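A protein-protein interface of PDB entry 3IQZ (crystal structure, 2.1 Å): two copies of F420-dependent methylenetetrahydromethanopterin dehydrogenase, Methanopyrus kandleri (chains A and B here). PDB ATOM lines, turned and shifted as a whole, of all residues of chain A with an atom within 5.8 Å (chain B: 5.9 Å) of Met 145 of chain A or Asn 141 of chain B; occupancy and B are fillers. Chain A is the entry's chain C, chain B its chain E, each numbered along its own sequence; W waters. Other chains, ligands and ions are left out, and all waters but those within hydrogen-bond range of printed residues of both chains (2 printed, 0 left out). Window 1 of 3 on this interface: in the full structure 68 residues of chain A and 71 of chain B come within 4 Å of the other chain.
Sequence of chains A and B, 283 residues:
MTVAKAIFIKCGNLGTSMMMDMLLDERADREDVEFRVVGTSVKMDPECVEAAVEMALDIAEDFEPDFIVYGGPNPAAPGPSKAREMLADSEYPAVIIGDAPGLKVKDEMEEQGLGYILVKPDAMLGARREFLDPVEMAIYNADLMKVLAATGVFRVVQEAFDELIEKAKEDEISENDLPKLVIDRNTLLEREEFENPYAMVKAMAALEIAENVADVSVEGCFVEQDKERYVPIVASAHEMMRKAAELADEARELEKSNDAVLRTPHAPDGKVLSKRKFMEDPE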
ATOM      1  N   GLY A  15     -14.649  -9.425  13.742  1.00  0.00           N
ATOM      2  CA  GLY A  15     -14.650  -8.917  15.130  1.00  0.00           C
ATOM      3  C   GLY A  15     -13.251  -8.431  15.536  1.00  0.00           C
ATOM      4  O   GLY A  15     -13.074  -7.378  16.192  1.00  0.00           O
ATOM      5  N   MET A  18     -11.998  -5.172  13.872  1.00  0.00           N
ATOM      6  CA  MET A  18     -12.723  -3.985  14.303  1.00  0.00           C
ATOM      7  C   MET A  18     -12.133  -3.407  15.622  1.00  0.00           C
ATOM      8  O   MET A  18     -12.031  -2.173  15.758  1.00  0.00           O
ATOM      9  CB  MET A  18     -14.224  -4.314  14.326  1.00  0.00           C
ATOM     10  CG  MET A  18     -15.134  -3.484  15.198  1.00  0.00           C
ATOM     11  SD  MET A  18     -16.826  -4.117  14.864  1.00  0.00           S
ATOM     12  CE  MET A  18     -17.453  -2.696  14.006  1.00  0.00           C
ATOM     13  N   MET A  19     -11.641  -4.273  16.516  1.00  0.00           N
ATOM     14  CA  MET A  19     -11.183  -3.874  17.859  1.00  0.00           C
ATOM     15  C   MET A  19      -9.660  -3.875  18.044  1.00  0.00           C
ATOM     16  O   MET A  19      -9.130  -3.367  19.071  1.00  0.00           O
ATOM     17  CB  MET A  19     -11.804  -4.798  18.934  1.00  0.00           C
ATOM     18  CG  MET A  19     -13.326  -4.518  19.203  1.00  0.00           C
ATOM     19  SD  MET A  19     -13.332  -3.138  20.403  1.00  0.00           S
ATOM     20  CE  MET A  19     -12.124  -3.820  21.473  1.00  0.00           C
ATOM     21  N   TYR A 140     -25.184  -9.116  15.211  1.00  0.00           N
ATOM     22  CA  TYR A 140     -24.264 -10.229  15.124  1.00  0.00           C
ATOM     23  C   TYR A 140     -22.901  -9.819  15.642  1.00  0.00           C
ATOM     24  O   TYR A 140     -22.228 -10.539  16.385  1.00  0.00           O
ATOM     25  CB  TYR A 140     -24.159 -10.698  13.683  1.00  0.00           C
ATOM     26  CG  TYR A 140     -23.158 -11.799  13.489  1.00  0.00           C
ATOM     27  CD1 TYR A 140     -23.565 -13.167  13.524  1.00  0.00           C
ATOM     28  CD2 TYR A 140     -21.827 -11.501  13.249  1.00  0.00           C
ATOM     29  CE1 TYR A 140     -22.637 -14.186  13.344  1.00  0.00           C
ATOM     30  CE2 TYR A 140     -20.881 -12.523  13.054  1.00  0.00           C
ATOM     31  CZ  TYR A 140     -21.313 -13.863  13.106  1.00  0.00           C
ATOM     32  OH  TYR A 140     -20.373 -14.869  12.924  1.00  0.00           O
ATOM     33  N   ASN A 141     -22.462  -8.639  15.231  1.00  0.00           N
ATOM     34  CA  ASN A 141     -21.186  -8.160  15.712  1.00  0.00           C
ATOM     35  C   ASN A 141     -21.145  -7.922  17.249  1.00  0.00           C
ATOM     36  O   ASN A 141     -20.123  -8.100  17.901  1.00  0.00           O
ATOM     37  CB  ASN A 141     -20.793  -6.893  14.920  1.00  0.00           C
ATOM     38  CG  ASN A 141     -20.097  -7.232  13.635  1.00  0.00           C
ATOM     39  OD1 ASN A 141     -18.867  -7.478  13.622  1.00  0.00           O
ATOM     40  ND2 ASN A 141     -20.867  -7.261  12.524  1.00  0.00           N
ATOM     41  N   ALA A 142     -22.266  -7.540  17.843  1.00  0.00           N
ATOM     42  CA  ALA A 142     -22.323  -7.415  19.308  1.00  0.00           C
ATOM     43  C   ALA A 142     -22.155  -8.771  20.021  1.00  0.00           C
ATOM     44  O   ALA A 142     -21.366  -8.914  20.979  1.00  0.00           O
ATOM     45  CB  ALA A 142     -23.578  -6.750  19.740  1.00  0.00           C
ATOM     46  N   ASP A 143     -22.818  -9.756  19.525  1.00  0.00           N
ATOM     47  CA  ASP A 143     -22.709 -11.109  20.072  1.00  0.00           C
ATOM     48  C   ASP A 143     -21.294 -11.645  19.846  1.00  0.00           C
ATOM     49  O   ASP A 143     -20.696 -12.203  20.733  1.00  0.00           O
ATOM     50  CB  ASP A 143     -23.728 -12.018  19.407  1.00  0.00           C
ATOM     51  CG  ASP A 143     -25.171 -11.779  19.913  1.00  0.00           C
ATOM     52  OD1 ASP A 143     -25.344 -11.247  21.023  1.00  0.00           O
ATOM     53  OD2 ASP A 143     -26.155 -12.160  19.204  1.00  0.00           O
ATOM     54  N   LEU A 144     -20.725 -11.383  18.670  1.00  0.00           N
ATOM     55  CA  LEU A 144     -19.423 -11.925  18.398  1.00  0.00           C
ATOM     56  C   LEU A 144     -18.346 -11.205  19.284  1.00  0.00           C
ATOM     57  O   LEU A 144     -17.390 -11.825  19.785  1.00  0.00           O
ATOM     58  CB  LEU A 144     -19.141 -11.874  16.909  1.00  0.00           C
ATOM     59  CG  LEU A 144     -17.681 -12.134  16.580  1.00  0.00           C
ATOM     60  CD1 LEU A 144     -17.298 -13.569  16.740  1.00  0.00           C
ATOM     61  CD2 LEU A 144     -17.423 -11.676  15.145  1.00  0.00           C
ATOM     62  N   MET A 145     -18.535  -9.912  19.511  1.00  0.00           N
ATOM     63  CA  MET A 145     -17.536  -9.152  20.264  1.00  0.00           C
ATOM     64  C   MET A 145     -17.492  -9.663  21.707  1.00  0.00           C
ATOM     65  O   MET A 145     -16.431  -9.839  22.311  1.00  0.00           O
ATOM     66  CB  MET A 145     -17.865  -7.665  20.241  1.00  0.00           C
ATOM     67  CG  MET A 145     -16.826  -6.819  20.927  1.00  0.00           C
ATOM     68  SD  MET A 145     -17.231  -5.058  20.773  1.00  0.00           S
ATOM     69  CE  MET A 145     -16.843  -4.650  19.086  1.00  0.00           C
ATOM     70  N   LYS A 146     -18.664  -9.849  22.263  1.00  0.00           N
ATOM     71  CA  LYS A 146     -18.847 -10.485  23.547  1.00  0.00           C
ATOM     72  C   LYS A 146     -18.130 -11.841  23.638  1.00  0.00           C
ATOM     73  O   LYS A 146     -17.391 -12.128  24.615  1.00  0.00           O
ATOM     74  CB  LYS A 146     -20.366 -10.656  23.834  1.00  0.00           C
ATOM     75  CG  LYS A 146     -20.679 -11.293  25.155  1.00  0.00           C
ATOM     76  CD  LYS A 146     -20.001 -10.479  26.255  1.00  0.00           C
ATOM     77  CE  LYS A 146     -20.623 -10.843  27.586  1.00  0.00           C
ATOM     78  NZ  LYS A 146     -21.968 -10.282  27.585  1.00  0.00           N
ATOM     79  N   VAL A 147     -18.421 -12.710  22.673  1.00  0.00           N
ATOM     80  CA  VAL A 147     -17.683 -13.963  22.625  1.00  0.00           C
ATOM     81  C   VAL A 147     -16.148 -13.735  22.648  1.00  0.00           C
ATOM     82  O   VAL A 147     -15.464 -14.372  23.447  1.00  0.00           O
ATOM     83  CB  VAL A 147     -18.017 -14.748  21.400  1.00  0.00           C
ATOM     84  CG1 VAL A 147     -17.099 -15.966  21.305  1.00  0.00           C
ATOM     85  CG2 VAL A 147     -19.491 -15.312  21.525  1.00  0.00           C
ATOM     86  N   LEU A 148     -15.628 -12.898  21.736  1.00  0.00           N
ATOM     87  CA  LEU A 148     -14.197 -12.816  21.577  1.00  0.00           C
ATOM     88  C   LEU A 148     -13.586 -12.092  22.775  1.00  0.00           C
ATOM     89  O   LEU A 148     -12.448 -12.388  23.122  1.00  0.00           O
ATOM     90  CB  LEU A 148     -13.774 -12.106  20.291  1.00  0.00           C
ATOM     91  CG  LEU A 148     -14.247 -12.770  18.990  1.00  0.00           C
ATOM     92  CD1 LEU A 148     -13.881 -11.919  17.775  1.00  0.00           C
ATOM     93  CD2 LEU A 148     -13.705 -14.181  18.837  1.00  0.00           C
ATOM     94  N   ALA A 149     -14.342 -11.186  23.405  1.00  0.00           N
ATOM     95  CA  ALA A 149     -13.860 -10.533  24.642  1.00  0.00           C
ATOM     96  C   ALA A 149     -13.890 -11.419  25.886  1.00  0.00           C
ATOM     97  O   ALA A 149     -12.852 -11.656  26.538  1.00  0.00           O
ATOM     98  CB  ALA A 149     -14.562  -9.156  24.899  1.00  0.00           C
ATOM     99  N   ALA A 150     -15.050 -11.918  26.206  1.00  0.00           N
ATOM    100  CA  ALA A 150     -15.229 -12.631  27.458  1.00  0.00           C
ATOM    101  C   ALA A 150     -14.562 -13.988  27.500  1.00  0.00           C
ATOM    102  O   ALA A 150     -14.357 -14.511  28.561  1.00  0.00           O
ATOM    103  CB  ALA A 150     -16.755 -12.712  27.874  1.00  0.00           C
ATOM    104  N   PHE A 154      -9.504 -11.790  22.977  1.00  0.00           N
ATOM    105  CA  PHE A 154      -8.984 -10.454  22.742  1.00  0.00           C
ATOM    106  C   PHE A 154      -7.757 -10.244  23.613  1.00  0.00           C
ATOM    107  O   PHE A 154      -6.881  -9.501  23.250  1.00  0.00           O
ATOM    108  CB  PHE A 154     -10.017  -9.345  23.018  1.00  0.00           C
ATOM    109  CG  PHE A 154     -10.982  -9.110  21.870  1.00  0.00           C
ATOM    110  CD1 PHE A 154     -12.203  -8.438  22.069  1.00  0.00           C
ATOM    111  CD2 PHE A 154     -10.666  -9.558  20.592  1.00  0.00           C
ATOM    112  CE1 PHE A 154     -13.102  -8.228  21.004  1.00  0.00           C
ATOM    113  CE2 PHE A 154     -11.555  -9.363  19.533  1.00  0.00           C
ATOM    114  CZ  PHE A 154     -12.768  -8.691  19.732  1.00  0.00           C
ATOM    115  N   ASN B  13     -13.608   6.604  20.576  1.00  0.00           N
ATOM    116  CA  ASN B  13     -14.607   5.631  20.196  1.00  0.00           C
ATOM    117  C   ASN B  13     -15.972   5.870  20.826  1.00  0.00           C
ATOM    118  O   ASN B  13     -16.129   6.080  22.045  1.00  0.00           O
ATOM    119  CB  ASN B  13     -14.152   4.206  20.602  1.00  0.00           C
ATOM    120  CG  ASN B  13     -14.993   3.098  19.915  1.00  0.00           C
ATOM    121  OD1 ASN B  13     -14.998   2.996  18.671  1.00  0.00           O
ATOM    122  ND2 ASN B  13     -15.734   2.306  20.716  1.00  0.00           N
ATOM    123  N   LEU B  14     -16.984   5.680  19.984  1.00  0.00           N
ATOM    124  CA  LEU B  14     -18.386   5.613  20.365  1.00  0.00           C
ATOM    125  C   LEU B  14     -18.977   4.396  19.645  1.00  0.00           C
ATOM    126  O   LEU B  14     -18.455   3.965  18.611  1.00  0.00           O
ATOM    127  CB  LEU B  14     -19.047   6.890  19.839  1.00  0.00           C
ATOM    128  CG  LEU B  14     -19.536   8.073  20.694  1.00  0.00           C
ATOM    129  CD1 LEU B  14     -18.947   8.226  22.106  1.00  0.00           C
ATOM    130  CD2 LEU B  14     -19.588   9.260  19.910  1.00  0.00           C
ATOM    131  N   GLY B  15     -20.043   3.820  20.178  1.00  0.00           N
ATOM    132  CA  GLY B  15     -20.692   2.726  19.499  1.00  0.00           C
ATOM    133  C   GLY B  15     -21.138   3.165  18.114  1.00  0.00           C
ATOM    134  O   GLY B  15     -21.016   2.416  17.152  1.00  0.00           O
ATOM    135  N   MET B  18     -18.257   3.738  15.695  1.00  0.00           N
ATOM    136  CA  MET B  18     -17.552   2.530  15.359  1.00  0.00           C
ATOM    137  C   MET B  18     -18.260   1.818  14.187  1.00  0.00           C
ATOM    138  O   MET B  18     -17.619   1.223  13.332  1.00  0.00           O
ATOM    139  CB  MET B  18     -17.355   1.676  16.609  1.00  0.00           C
ATOM    140  CG  MET B  18     -17.183   0.211  16.420  1.00  0.00           C
ATOM    141  SD  MET B  18     -16.793  -0.537  18.029  1.00  0.00           S
ATOM    142  CE  MET B  18     -15.074  -0.801  17.828  1.00  0.00           C
ATOM    143  N   LEU B 125     -17.985   4.897  28.860  1.00  0.00           N
ATOM    144  CA  LEU B 125     -17.789   3.732  29.767  1.00  0.00           C
ATOM    145  C   LEU B 125     -16.924   4.129  30.990  1.00  0.00           C
ATOM    146  O   LEU B 125     -16.569   5.275  31.123  1.00  0.00           O
ATOM    147  CB  LEU B 125     -17.165   2.552  29.031  1.00  0.00           C
ATOM    148  CG  LEU B 125     -15.997   3.010  28.148  1.00  0.00           C
ATOM    149  CD1 LEU B 125     -14.844   3.690  28.924  1.00  0.00           C
ATOM    150  CD2 LEU B 125     -15.559   1.734  27.399  1.00  0.00           C
ATOM    151  N   GLU B 136     -12.601  -5.612  29.170  1.00  0.00           N
ATOM    152  CA  GLU B 136     -13.804  -4.997  29.766  1.00  0.00           C
ATOM    153  C   GLU B 136     -14.353  -3.889  28.849  1.00  0.00           C
ATOM    154  O   GLU B 136     -15.588  -3.676  28.736  1.00  0.00           O
ATOM    155  CB  GLU B 136     -13.480  -4.395  31.149  1.00  0.00           C
ATOM    156  CG  GLU B 136     -14.664  -3.667  31.793  1.00  0.00           C
ATOM    157  CD  GLU B 136     -15.778  -4.656  32.196  1.00  0.00           C
ATOM    158  OE1 GLU B 136     -16.952  -4.322  31.965  1.00  0.00           O
ATOM    159  OE2 GLU B 136     -15.463  -5.701  32.777  1.00  0.00           O
ATOM    160  N   MET B 137     -13.435  -3.210  28.177  1.00  0.00           N
ATOM    161  CA  MET B 137     -13.775  -2.191  27.219  1.00  0.00           C
ATOM    162  C   MET B 137     -14.516  -2.786  26.021  1.00  0.00           C
ATOM    163  O   MET B 137     -15.537  -2.242  25.584  1.00  0.00           O
ATOM    164  CB  MET B 137     -12.498  -1.431  26.783  1.00  0.00           C
ATOM    165  CG  MET B 137     -12.684  -0.425  25.691  1.00  0.00           C
ATOM    166  SD  MET B 137     -12.660  -1.118  24.006  1.00  0.00           S
ATOM    167  CE  MET B 137     -11.016  -1.761  23.761  1.00  0.00           C
ATOM    168  N   ALA B 138     -14.036  -3.928  25.528  1.00  0.00           N
ATOM    169  CA  ALA B 138     -14.740  -4.694  24.486  1.00  0.00           C
ATOM    170  C   ALA B 138     -16.106  -5.248  24.955  1.00  0.00           C
ATOM    171  O   ALA B 138     -17.092  -5.284  24.181  1.00  0.00           O
ATOM    172  CB  ALA B 138     -13.865  -5.850  24.041  1.00  0.00           C
ATOM    173  N   ILE B 139     -16.170  -5.728  26.190  1.00  0.00           N
ATOM    174  CA  ILE B 139     -17.429  -6.253  26.684  1.00  0.00           C
ATOM    175  C   ILE B 139     -18.473  -5.156  26.711  1.00  0.00           C
ATOM    176  O   ILE B 139     -19.611  -5.323  26.283  1.00  0.00           O
ATOM    177  CB  ILE B 139     -17.272  -6.906  28.074  1.00  0.00           C
ATOM    178  CG1 ILE B 139     -16.309  -8.094  27.949  1.00  0.00           C
ATOM    179  CG2 ILE B 139     -18.705  -7.376  28.701  1.00  0.00           C
ATOM    180  CD1 ILE B 139     -16.126  -8.923  29.234  1.00  0.00           C
ATOM    181  N   TYR B 140     -18.070  -3.994  27.182  1.00  0.00           N
ATOM    182  CA  TYR B 140     -19.004  -2.911  27.256  1.00  0.00           C
ATOM    183  C   TYR B 140     -19.470  -2.561  25.862  1.00  0.00           C
ATOM    184  O   TYR B 140     -20.640  -2.259  25.633  1.00  0.00           O
ATOM    185  CB  TYR B 140     -18.297  -1.715  27.898  1.00  0.00           C
ATOM    186  CG  TYR B 140     -19.130  -0.466  27.919  1.00  0.00           C
ATOM    187  CD1 TYR B 140     -19.902  -0.161  29.019  1.00  0.00           C
ATOM    188  CD2 TYR B 140     -19.173   0.375  26.825  1.00  0.00           C
ATOM    189  CE1 TYR B 140     -20.690   0.957  29.064  1.00  0.00           C
ATOM    190  CE2 TYR B 140     -19.926   1.569  26.868  1.00  0.00           C
ATOM    191  CZ  TYR B 140     -20.686   1.846  28.006  1.00  0.00           C
ATOM    192  OH  TYR B 140     -21.476   2.980  28.093  1.00  0.00           O
ATOM    193  N   ASN B 141     -18.490  -2.435  24.950  1.00  0.00           N
ATOM    194  CA  ASN B 141     -18.789  -2.078  23.593  1.00  0.00           C
ATOM    195  C   ASN B 141     -19.775  -3.111  22.997  1.00  0.00           C
ATOM    196  O   ASN B 141     -20.659  -2.756  22.215  1.00  0.00           O
ATOM    197  CB  ASN B 141     -17.499  -1.937  22.803  1.00  0.00           C
ATOM    198  CG  ASN B 141     -17.033  -0.479  22.737  1.00  0.00           C
ATOM    199  OD1 ASN B 141     -17.585   0.307  21.971  1.00  0.00           O
ATOM    200  ND2 ASN B 141     -16.041  -0.112  23.567  1.00  0.00           N
ATOM    201  N   ALA B 142     -19.637  -4.376  23.371  1.00  0.00           N
ATOM    202  CA  ALA B 142     -20.551  -5.420  22.914  1.00  0.00           C
ATOM    203  C   ALA B 142     -22.017  -5.219  23.380  1.00  0.00           C
ATOM    204  O   ALA B 142     -22.945  -5.400  22.602  1.00  0.00           O
ATOM    205  CB  ALA B 142     -20.059  -6.821  23.351  1.00  0.00           C
ATOM    206  N   ASP B 143     -22.198  -4.836  24.647  1.00  0.00           N
ATOM    207  CA  ASP B 143     -23.526  -4.575  25.184  1.00  0.00           C
ATOM    208  C   ASP B 143     -24.075  -3.267  24.571  1.00  0.00           C
ATOM    209  O   ASP B 143     -25.243  -3.197  24.143  1.00  0.00           O
ATOM    210  CB  ASP B 143     -23.437  -4.476  26.709  1.00  0.00           C
ATOM    211  CG  ASP B 143     -23.213  -5.853  27.382  1.00  0.00           C
ATOM    212  OD1 ASP B 143     -23.693  -6.830  26.811  1.00  0.00           O
ATOM    213  OD2 ASP B 143     -22.529  -5.991  28.450  1.00  0.00           O
ATOM    214  N   LEU B 144     -23.251  -2.226  24.496  1.00  0.00           N
ATOM    215  CA  LEU B 144     -23.700  -1.000  23.870  1.00  0.00           C
ATOM    216  C   LEU B 144     -24.175  -1.239  22.416  1.00  0.00           C
ATOM    217  O   LEU B 144     -25.201  -0.715  21.978  1.00  0.00           O
ATOM    218  CB  LEU B 144     -22.592   0.042  23.896  1.00  0.00           C
ATOM    219  CG  LEU B 144     -22.950   1.350  23.207  1.00  0.00           C
ATOM    220  CD1 LEU B 144     -24.167   1.953  23.922  1.00  0.00           C
ATOM    221  CD2 LEU B 144     -21.736   2.360  23.188  1.00  0.00           C
ATOM    222  N   MET B 145     -23.405  -2.007  21.655  1.00  0.00           N
ATOM    223  CA  MET B 145     -23.722  -2.224  20.259  1.00  0.00           C
ATOM    224  C   MET B 145     -25.064  -2.929  20.101  1.00  0.00           C
ATOM    225  O   MET B 145     -25.876  -2.563  19.253  1.00  0.00           O
ATOM    226  CB  MET B 145     -22.593  -2.986  19.575  1.00  0.00           C
ATOM    227  CG  MET B 145     -22.899  -3.264  18.089  1.00  0.00           C
ATOM    228  SD  MET B 145     -21.523  -4.124  17.297  1.00  0.00           S
ATOM    229  CE  MET B 145     -20.189  -2.964  17.452  1.00  0.00           C
ATOM    230  N   LYS B 146     -25.308  -3.937  20.946  1.00  0.00           N
ATOM    231  CA  LYS B 146     -26.539  -4.622  21.016  1.00  0.00           C
ATOM    232  C   LYS B 146     -27.713  -3.686  21.298  1.00  0.00           C
ATOM    233  O   LYS B 146     -28.804  -3.796  20.704  1.00  0.00           O
ATOM    234  CB  LYS B 146     -26.422  -5.658  22.147  1.00  0.00           C
ATOM    235  CG  LYS B 146     -27.693  -6.560  22.306  1.00  0.00           C
ATOM    236  CD  LYS B 146     -28.142  -7.011  20.984  1.00  0.00           C
ATOM    237  CE  LYS B 146     -29.215  -7.997  21.203  1.00  0.00           C
ATOM    238  NZ  LYS B 146     -28.514  -9.164  21.813  1.00  0.00           N
HETATM  239  O   HOH W   1     -21.953  -8.063  29.566  1.00  0.00           O
HETATM  240  O   HOH W   2     -28.460 -11.526  19.645  1.00  0.00           O
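Among the printed residues, merely in contact across the chains: Ala 142 of chain A with Ala 142 of chain B (3.2 Å), Met 19 of chain A with Met 137 of chain B (3.3 Å), Ala 149 of chain A with Ala 138 of chain B (3.5 Å), Lys 146 of chain A with Ala 142 of chain B (3.5 Å), Ala 142 of chain A with Lys 146 of chain B (3.5 Å), Phe 154 of chain A with Ala 138 of chain B (3.7 Å), Ala 149 of chain A with Ile 139 of chain B (3.7 Å), Met 19 of chain A with Ala 138 of chain B (3.7 Å), Asn 141 of chain A with Met 145 of chain B (3.7 Å), Met 145 of chain A with Asn 141 of chain B (3.7 Å), Met 18 of chain A with Met 18 of chain B (3.8 Å) and Met 19 of chain A with Met 18 of chain B (3.9 Å).
Of the printed residues of chain B, Met 18 of chain A touches Met 18 (3.8 Å). Printed residues of chain B within 4 Å of Met 19 of chain A: Met 18, Met 137 and Ala 138. Of the printed residues of chain B, Ala 142 of chain A touches Ala 142, Met 145 and Lys 146. Met 145 of chain A touches just these residues of chain B: Ala 138, Asn 141 and Ala 142. Leu 14 of chain B touches none of the printed residues of chain A. Of chain A, only Met 145 comes within 4 Å of Asn 141 of chain B. Of the printed residues of chain A, Met 145 of chain B touches Asn 141 and Ala 142. The nearest residue of chain B that does not touch Met 145 of chain A is Met 145 of chain B (4.1 Å). The nearest residue of chain A that does not touch Asn 141 of chain B is Met 19 of chain A (5.0 Å).
Water W1 bridges the side-chain carboxylate (OD2) of Asp 143 of chain B (2.4 Å) and the side-chain amino group (NZ) of Lys 146 of chain A (3.0 Å). Water W2 bridges the side-chain carboxylate of Asp 143 of chain A (2.4 Å) and the side-chain amino group of Lys 146 of chain B (3.2 Å).
The backbone carbonyl oxygen of Leu 148 of chain A is in hydrogen-bond range of the backbone NH of Phe 154 of chain A (3.0 Å). O of Met 137 of chain B sits at hydrogen-bond distance from ND2 of Asn 141 of chain B (3.0 Å). The side-chain amide nitrogen (ND2) of Asn 13 of chain B is in hydrogen-bond range of the side-chain amide oxygen (OD1) of Asn 141 of chain B (3.0 Å).
The side-chain amino group (NZ) of Lys 146 of chain B is in salt-bridge range of the side-chain carboxylate (OD1) of Asp 143 of chain A (3.9 Å). The side-chain sulfur of Met 145 of chain A sits at hydrogen-bond distance from the backbone NH of Ala 142 of chain B (3.6 Å). The backbone carbonyl oxygen (O) of Ala 138 of chain B sits close to the side-chain sulfur (SD) of Met 145 of chain A. The backbone NH (N) of Ala 142 of chain A sits at hydrogen-bond distance from the side-chain sulfur (SD) of Met 145 of chain B (3.5 Å). NZ of Lys 146 of chain A is in salt-bridge range of OD1 of Asp 143 of chain B, at 3.9 Å.
Of the 16 printed residues of chain B, 9 touch a printed residue of chain A. Hydrophobic or aromatic side chains of chain B that line the printed part of chain A: Met 18, Met 137, Ala 138, Ile 139, Ala 142 and Met 145. Of the 15 printed residues of chain A, 9 touch a printed residue of chain B. Among the printed residues, Asp or Glu carboxylates within 4 Å of a Lys or Arg side-chain nitrogen of the other chain: Asp 143 of chain A with Lys 146 of chain B and Lys 146 of chain A with Asp 143 of chain B.
Met 18 of chain A touches its own counterpart, Met 18 of chain B. Asn 141 of chain A touches Met 145 of chain B, and with the chains exchanged Met 145 of chain A touches Asn 141 of chain B. Ala 142 of chain A touches Met 145 of chain B, and with the chains exchanged Met 145 of chain A touches Ala 142 of chain B. Asp 143 of chain A touches Lys 146 of chain B, and with the chains exchanged Lys 146 of chain A touches Asp 143 of chain B.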
